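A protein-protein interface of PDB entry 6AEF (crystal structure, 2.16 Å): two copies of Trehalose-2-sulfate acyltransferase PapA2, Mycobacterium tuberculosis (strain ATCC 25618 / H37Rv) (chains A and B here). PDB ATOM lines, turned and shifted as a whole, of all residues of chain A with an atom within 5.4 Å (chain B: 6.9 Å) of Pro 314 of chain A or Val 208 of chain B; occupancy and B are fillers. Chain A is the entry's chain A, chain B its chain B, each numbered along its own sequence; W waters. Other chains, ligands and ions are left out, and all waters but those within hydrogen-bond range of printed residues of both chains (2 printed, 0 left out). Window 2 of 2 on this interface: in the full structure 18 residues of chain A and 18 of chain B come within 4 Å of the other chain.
No position is printed for both chains.
Hydrophobic or aromatic side chains of chain B within 4 Å of the printed part of chain A: Val 208 and Ala 212. Hydrophobic or aromatic side chains of chain A within 4 Å of the printed part of chain B: Pro 314.
Of chain A, only Pro 314 comes within 4 Å of Val 208 of chain B. Of the printed residues of chain B, Thr 313 of chain A touches Arg 209 (3.6 Å). Of the printed residues of chain A, Ala 212 of chain B touches Arg 312. The nearest residue of chain B that does not touch Pro 314 of chain A is Ala 212 of chain B (6.1 Å).
Water W2 lies within hydrogen-bond range of OG1 of Thr 313 of chain A (2.5 Å) and NH2 of Arg 209 of chain B (2.9 Å). Water W1 bridges O of Asp 213 of chain B and NH1 of Arg 312 of chain A.
OE2 of Glu 316 of chain A is in salt-bridge range of NH1 of Arg 209 of chain B. The side-chain carboxylate of Asp 213 of chain B is in salt-bridge range of the guanidinium group of Arg 312 of chain A, at 3.2 Å.
The backbone NH (N) of Arg 312 of chain A is in hydrogen-bond range of the side-chain carboxylate (OE1) of Glu 316 of chain A (2.7 Å). The backbone NH of Thr 313 of chain A is in hydrogen-bond range of the side-chain carboxylate of Glu 316 of chain A (3.0 Å).
O of Arg 312 of chain A touches CB of Ala 212 of chain B, at 3.8 Å. CG2 of Thr 313 of chain A touches CZ of Arg 209 of chain B, at 3.6 Å. Val 208 of chain B touches Pro 314 of chain A.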
ATOM      1  N   ARG A 312      -8.629   3.985  -0.965  1.00  0.00           N
ATOM      2  CA  ARG A 312      -8.558   2.909   0.020  1.00  0.00           C
ATOM      3  C   ARG A 312      -9.836   2.085   0.154  1.00  0.00           C
ATOM      4  O   ARG A 312      -9.766   0.853   0.187  1.00  0.00           O
ATOM      5  CB  ARG A 312      -8.163   3.488   1.375  1.00  0.00           C
ATOM      6  CG  ARG A 312      -6.665   3.660   1.480  1.00  0.00           C
ATOM      7  CD  ARG A 312      -6.270   4.407   2.702  1.00  0.00           C
ATOM      8  NE  ARG A 312      -4.859   4.770   2.662  1.00  0.00           N
ATOM      9  CZ  ARG A 312      -4.248   5.471   3.608  1.00  0.00           C
ATOM     10  NH1 ARG A 312      -4.925   5.880   4.668  1.00  0.00           N
ATOM     11  NH2 ARG A 312      -2.961   5.760   3.495  1.00  0.00           N
ATOM     12  N   THR A 313     -10.994   2.731   0.238  1.00  0.00           N
ATOM     13  CA  THR A 313     -12.251   2.010   0.368  1.00  0.00           C
ATOM     14  C   THR A 313     -12.702   1.464  -0.981  1.00  0.00           C
ATOM     15  O   THR A 313     -12.252   1.924  -2.031  1.00  0.00           O
ATOM     16  CB  THR A 313     -13.340   2.923   0.918  1.00  0.00           C
ATOM     17  OG1 THR A 313     -13.638   3.934  -0.049  1.00  0.00           O
ATOM     18  CG2 THR A 313     -12.888   3.576   2.204  1.00  0.00           C
ATOM     19  N   PRO A 314     -13.588   0.470  -0.982  1.00  0.00           N
ATOM     20  CA  PRO A 314     -14.148   0.010  -2.261  1.00  0.00           C
ATOM     21  C   PRO A 314     -14.732   1.134  -3.092  1.00  0.00           C
ATOM     22  O   PRO A 314     -14.561   1.158  -4.315  1.00  0.00           O
ATOM     23  CB  PRO A 314     -15.217  -0.999  -1.826  1.00  0.00           C
ATOM     24  CG  PRO A 314     -14.724  -1.511  -0.508  1.00  0.00           C
ATOM     25  CD  PRO A 314     -14.079  -0.329   0.155  1.00  0.00           C
ATOM     26  N   THR A 315     -15.419   2.077  -2.452  1.00  0.00           N
ATOM     27  CA  THR A 315     -16.041   3.173  -3.189  1.00  0.00           C
ATOM     28  C   THR A 315     -14.986   4.060  -3.843  1.00  0.00           C
ATOM     29  O   THR A 315     -15.140   4.470  -4.998  1.00  0.00           O
ATOM     30  CB  THR A 315     -16.939   3.976  -2.238  1.00  0.00           C
ATOM     31  OG1 THR A 315     -18.100   3.197  -1.914  1.00  0.00           O
ATOM     32  CG2 THR A 315     -17.407   5.260  -2.878  1.00  0.00           C
ATOM     33  N   GLU A 316     -13.903   4.359  -3.123  1.00  0.00           N
ATOM     34  CA  GLU A 316     -12.824   5.145  -3.708  1.00  0.00           C
ATOM     35  C   GLU A 316     -12.160   4.399  -4.862  1.00  0.00           C
ATOM     36  O   GLU A 316     -11.775   5.007  -5.869  1.00  0.00           O
ATOM     37  CB  GLU A 316     -11.805   5.490  -2.631  1.00  0.00           C
ATOM     38  CG  GLU A 316     -12.322   6.483  -1.617  1.00  0.00           C
ATOM     39  CD  GLU A 316     -11.438   6.582  -0.391  1.00  0.00           C
ATOM     40  OE1 GLU A 316     -10.580   5.694  -0.201  1.00  0.00           O
ATOM     41  OE2 GLU A 316     -11.599   7.551   0.380  1.00  0.00           O
ATOM     42  N   LEU A 317     -12.026   3.074  -4.735  1.00  0.00           N
ATOM     43  CA  LEU A 317     -11.451   2.285  -5.818  1.00  0.00           C
ATOM     44  C   LEU A 317     -12.317   2.347  -7.065  1.00  0.00           C
ATOM     45  O   LEU A 317     -11.810   2.165  -8.176  1.00  0.00           O
ATOM     46  CB  LEU A 317     -11.242   0.834  -5.367  1.00  0.00           C
ATOM     47  CG  LEU A 317     -10.121   0.660  -4.341  1.00  0.00           C
ATOM     48  CD1 LEU A 317     -10.157  -0.719  -3.679  1.00  0.00           C
ATOM     49  CD2 LEU A 317      -8.765   0.881  -4.985  1.00  0.00           C
ATOM     50  N   ARG A 318     -13.614   2.616  -6.912  1.00  0.00           N
ATOM     51  CA  ARG A 318     -14.504   2.783  -8.053  1.00  0.00           C
ATOM     52  C   ARG A 318     -14.713   4.245  -8.421  1.00  0.00           C
ATOM     53  O   ARG A 318     -15.697   4.565  -9.096  1.00  0.00           O
ATOM     54  CB  ARG A 318     -15.864   2.149  -7.777  1.00  0.00           C
ATOM     55  CG  ARG A 318     -15.835   0.671  -7.443  1.00  0.00           C
ATOM     56  CD  ARG A 318     -17.255   0.133  -7.399  1.00  0.00           C
ATOM     57  NE  ARG A 318     -18.000   0.625  -6.239  1.00  0.00           N
ATOM     58  CZ  ARG A 318     -18.129   0.002  -5.073  1.00  0.00           C
ATOM     59  NH1 ARG A 318     -17.565  -1.180  -4.856  1.00  0.00           N
ATOM     60  NH2 ARG A 318     -18.834   0.580  -4.111  1.00  0.00           N
ATOM     61  N   GLU B  37     -19.498  -9.146   5.162  1.00  0.00           N
ATOM     62  CA  GLU B  37     -18.054  -8.956   5.062  1.00  0.00           C
ATOM     63  C   GLU B  37     -17.578  -7.681   5.752  1.00  0.00           C
ATOM     64  O   GLU B  37     -16.369  -7.423   5.776  1.00  0.00           O
ATOM     65  CB  GLU B  37     -17.622  -8.949   3.592  1.00  0.00           C
ATOM     66  CG  GLU B  37     -17.609 -10.333   2.938  1.00  0.00           C
ATOM     67  CD  GLU B  37     -17.107 -10.306   1.502  1.00  0.00           C
ATOM     68  OE1 GLU B  37     -17.745  -9.633   0.666  1.00  0.00           O
ATOM     69  OE2 GLU B  37     -16.074 -10.953   1.208  1.00  0.00           O
ATOM     70  N   VAL B  38     -18.489  -6.865   6.280  1.00  0.00           N
ATOM     71  CA  VAL B  38     -18.116  -5.674   7.037  1.00  0.00           C
ATOM     72  C   VAL B  38     -17.651  -6.100   8.429  1.00  0.00           C
ATOM     73  O   VAL B  38     -18.420  -6.726   9.177  1.00  0.00           O
ATOM     74  CB  VAL B  38     -19.283  -4.681   7.120  1.00  0.00           C
ATOM     75  CG1 VAL B  38     -18.860  -3.434   7.896  1.00  0.00           C
ATOM     76  CG2 VAL B  38     -19.798  -4.326   5.717  1.00  0.00           C
ATOM     77  N   PRO B  39     -16.428  -5.780   8.835  1.00  0.00           N
ATOM     78  CA  PRO B  39     -15.977  -6.180  10.166  1.00  0.00           C
ATOM     79  C   PRO B  39     -16.579  -5.290  11.238  1.00  0.00           C
ATOM     80  O   PRO B  39     -17.155  -4.230  10.943  1.00  0.00           O
ATOM     81  CB  PRO B  39     -14.454  -6.005  10.090  1.00  0.00           C
ATOM     82  CG  PRO B  39     -14.269  -4.899   9.133  1.00  0.00           C
ATOM     83  CD  PRO B  39     -15.384  -5.032   8.108  1.00  0.00           C
ATOM     84  N   TYR B 203     -22.853   3.267   9.627  1.00  0.00           N
ATOM     85  CA  TYR B 203     -21.687   2.911  10.424  1.00  0.00           C
ATOM     86  C   TYR B 203     -20.871   1.798   9.772  1.00  0.00           C
ATOM     87  O   TYR B 203     -19.654   1.709   9.999  1.00  0.00           O
ATOM     88  CB  TYR B 203     -22.141   2.515  11.825  1.00  0.00           C
ATOM     89  CG  TYR B 203     -21.012   2.316  12.820  1.00  0.00           C
ATOM     90  CD1 TYR B 203     -20.350   3.402  13.372  1.00  0.00           C
ATOM     91  CD2 TYR B 203     -20.617   1.042  13.208  1.00  0.00           C
ATOM     92  CE1 TYR B 203     -19.317   3.228  14.288  1.00  0.00           C
ATOM     93  CE2 TYR B 203     -19.585   0.857  14.124  1.00  0.00           C
ATOM     94  CZ  TYR B 203     -18.942   1.956  14.655  1.00  0.00           C
ATOM     95  OH  TYR B 203     -17.927   1.778  15.565  1.00  0.00           O
ATOM     96  N   ASP B 204     -21.521   0.925   8.991  1.00  0.00           N
ATOM     97  CA  ASP B 204     -20.789  -0.056   8.193  1.00  0.00           C
ATOM     98  C   ASP B 204     -19.674   0.609   7.389  1.00  0.00           C
ATOM     99  O   ASP B 204     -18.540   0.116   7.346  1.00  0.00           O
ATOM    100  CB  ASP B 204     -21.742  -0.787   7.245  1.00  0.00           C
ATOM    101  CG  ASP B 204     -22.617  -1.801   7.948  1.00  0.00           C
ATOM    102  OD1 ASP B 204     -22.699  -1.770   9.196  1.00  0.00           O
ATOM    103  OD2 ASP B 204     -23.224  -2.641   7.243  1.00  0.00           O
ATOM    104  N   ASP B 205     -20.001   1.719   6.708  1.00  0.00           N
ATOM    105  CA  ASP B 205     -19.022   2.411   5.871  1.00  0.00           C
ATOM    106  C   ASP B 205     -17.830   2.848   6.696  1.00  0.00           C
ATOM    107  O   ASP B 205     -16.681   2.738   6.253  1.00  0.00           O
ATOM    108  CB  ASP B 205     -19.652   3.635   5.204  1.00  0.00           C
ATOM    109  CG  ASP B 205     -20.732   3.277   4.216  1.00  0.00           C
ATOM    110  OD1 ASP B 205     -20.928   2.075   3.952  1.00  0.00           O
ATOM    111  OD2 ASP B 205     -21.382   4.212   3.691  1.00  0.00           O
ATOM    112  N   HIS B 206     -18.089   3.336   7.908  1.00  0.00           N
ATOM    113  CA  HIS B 206     -17.001   3.720   8.791  1.00  0.00           C
ATOM    114  C   HIS B 206     -16.138   2.521   9.154  1.00  0.00           C
ATOM    115  O   HIS B 206     -14.911   2.637   9.215  1.00  0.00           O
ATOM    116  CB  HIS B 206     -17.543   4.367  10.067  1.00  0.00           C
ATOM    117  CG  HIS B 206     -16.486   4.597  11.100  1.00  0.00           C
ATOM    118  ND1 HIS B 206     -15.569   5.621  11.006  1.00  0.00           N
ATOM    119  CD2 HIS B 206     -16.161   3.901  12.217  1.00  0.00           C
ATOM    120  CE1 HIS B 206     -14.746   5.567  12.036  1.00  0.00           C
ATOM    121  NE2 HIS B 206     -15.081   4.532  12.785  1.00  0.00           N
ATOM    122  N   CYS B 207     -16.755   1.363   9.425  1.00  0.00           N
ATOM    123  CA  CYS B 207     -15.963   0.170   9.735  1.00  0.00           C
ATOM    124  C   CYS B 207     -15.040  -0.195   8.574  1.00  0.00           C
ATOM    125  O   CYS B 207     -13.847  -0.491   8.765  1.00  0.00           O
ATOM    126  CB  CYS B 207     -16.889  -0.998  10.081  1.00  0.00           C
ATOM    127  SG  CYS B 207     -17.913  -0.756  11.575  1.00  0.00           S
ATOM    128  N   VAL B 208     -15.574  -0.174   7.354  1.00  0.00           N
ATOM    129  CA  VAL B 208     -14.761  -0.489   6.174  1.00  0.00           C
ATOM    130  C   VAL B 208     -13.608   0.503   6.030  1.00  0.00           C
ATOM    131  O   VAL B 208     -12.448   0.118   5.819  1.00  0.00           O
ATOM    132  CB  VAL B 208     -15.647  -0.511   4.915  1.00  0.00           C
ATOM    133  CG1 VAL B 208     -14.810  -0.722   3.645  1.00  0.00           C
ATOM    134  CG2 VAL B 208     -16.698  -1.613   5.035  1.00  0.00           C
ATOM    135  N   ARG B 209     -13.911   1.801   6.117  1.00  0.00           N
ATOM    136  CA  ARG B 209     -12.862   2.803   5.965  1.00  0.00           C
ATOM    137  C   ARG B 209     -11.809   2.656   7.049  1.00  0.00           C
ATOM    138  O   ARG B 209     -10.613   2.774   6.781  1.00  0.00           O
ATOM    139  CB  ARG B 209     -13.451   4.209   6.011  1.00  0.00           C
ATOM    140  CG  ARG B 209     -12.388   5.297   5.953  1.00  0.00           C
ATOM    141  CD  ARG B 209     -13.020   6.662   5.782  1.00  0.00           C
ATOM    142  NE  ARG B 209     -13.797   6.744   4.557  1.00  0.00           N
ATOM    143  CZ  ARG B 209     -13.284   6.971   3.351  1.00  0.00           C
ATOM    144  NH1 ARG B 209     -11.980   7.140   3.197  1.00  0.00           N
ATOM    145  NH2 ARG B 209     -14.082   7.022   2.292  1.00  0.00           N
ATOM    146  N   GLN B 210     -12.240   2.421   8.287  1.00  0.00           N
ATOM    147  CA  GLN B 210     -11.296   2.293   9.386  1.00  0.00           C
ATOM    148  C   GLN B 210     -10.351   1.129   9.145  1.00  0.00           C
ATOM    149  O   GLN B 210      -9.140   1.255   9.347  1.00  0.00           O
ATOM    150  CB  GLN B 210     -12.053   2.107  10.707  1.00  0.00           C
ATOM    151  CG  GLN B 210     -11.193   1.738  11.896  1.00  0.00           C
ATOM    152  CD  GLN B 210     -12.018   1.537  13.166  1.00  0.00           C
ATOM    153  OE1 GLN B 210     -12.735   0.546  13.296  1.00  0.00           O
ATOM    154  NE2 GLN B 210     -11.919   2.479  14.098  1.00  0.00           N
ATOM    155  N   TYR B 211     -10.870  -0.001   8.673  1.00  0.00           N
ATOM    156  CA  TYR B 211      -9.959  -1.114   8.439  1.00  0.00           C
ATOM    157  C   TYR B 211      -9.021  -0.826   7.277  1.00  0.00           C
ATOM    158  O   TYR B 211      -7.824  -1.137   7.358  1.00  0.00           O
ATOM    159  CB  TYR B 211     -10.738  -2.400   8.227  1.00  0.00           C
ATOM    160  CG  TYR B 211     -11.041  -3.052   9.549  1.00  0.00           C
ATOM    161  CD1 TYR B 211     -11.936  -2.469  10.446  1.00  0.00           C
ATOM    162  CD2 TYR B 211     -10.405  -4.228   9.924  1.00  0.00           C
ATOM    163  CE1 TYR B 211     -12.205  -3.055  11.666  1.00  0.00           C
ATOM    164  CE2 TYR B 211     -10.669  -4.821  11.147  1.00  0.00           C
ATOM    165  CZ  TYR B 211     -11.571  -4.226  12.009  1.00  0.00           C
ATOM    166  OH  TYR B 211     -11.837  -4.810  13.218  1.00  0.00           O
ATOM    167  N   ALA B 212      -9.522  -0.188   6.212  1.00  0.00           N
ATOM    168  CA  ALA B 212      -8.640   0.184   5.106  1.00  0.00           C
ATOM    169  C   ALA B 212      -7.528   1.122   5.566  1.00  0.00           C
ATOM    170  O   ALA B 212      -6.370   0.966   5.164  1.00  0.00           O
ATOM    171  CB  ALA B 212      -9.447   0.824   3.977  1.00  0.00           C
ATOM    172  N   ASP B 213      -7.859   2.105   6.405  1.00  0.00           N
ATOM    173  CA  ASP B 213      -6.861   3.058   6.883  1.00  0.00           C
ATOM    174  C   ASP B 213      -5.849   2.394   7.815  1.00  0.00           C
ATOM    175  O   ASP B 213      -4.642   2.645   7.712  1.00  0.00           O
ATOM    176  CB  ASP B 213      -7.550   4.230   7.590  1.00  0.00           C
ATOM    177  CG  ASP B 213      -8.266   5.166   6.619  1.00  0.00           C
ATOM    178  OD1 ASP B 213      -7.982   5.106   5.403  1.00  0.00           O
ATOM    179  OD2 ASP B 213      -9.121   5.954   7.071  1.00  0.00           O
HETATM  180  O   HOH W   1      -4.009   5.235   7.515  1.00  0.00           O
HETATM  181  O   HOH W   2     -15.680   5.151   0.667  1.00  0.00           O
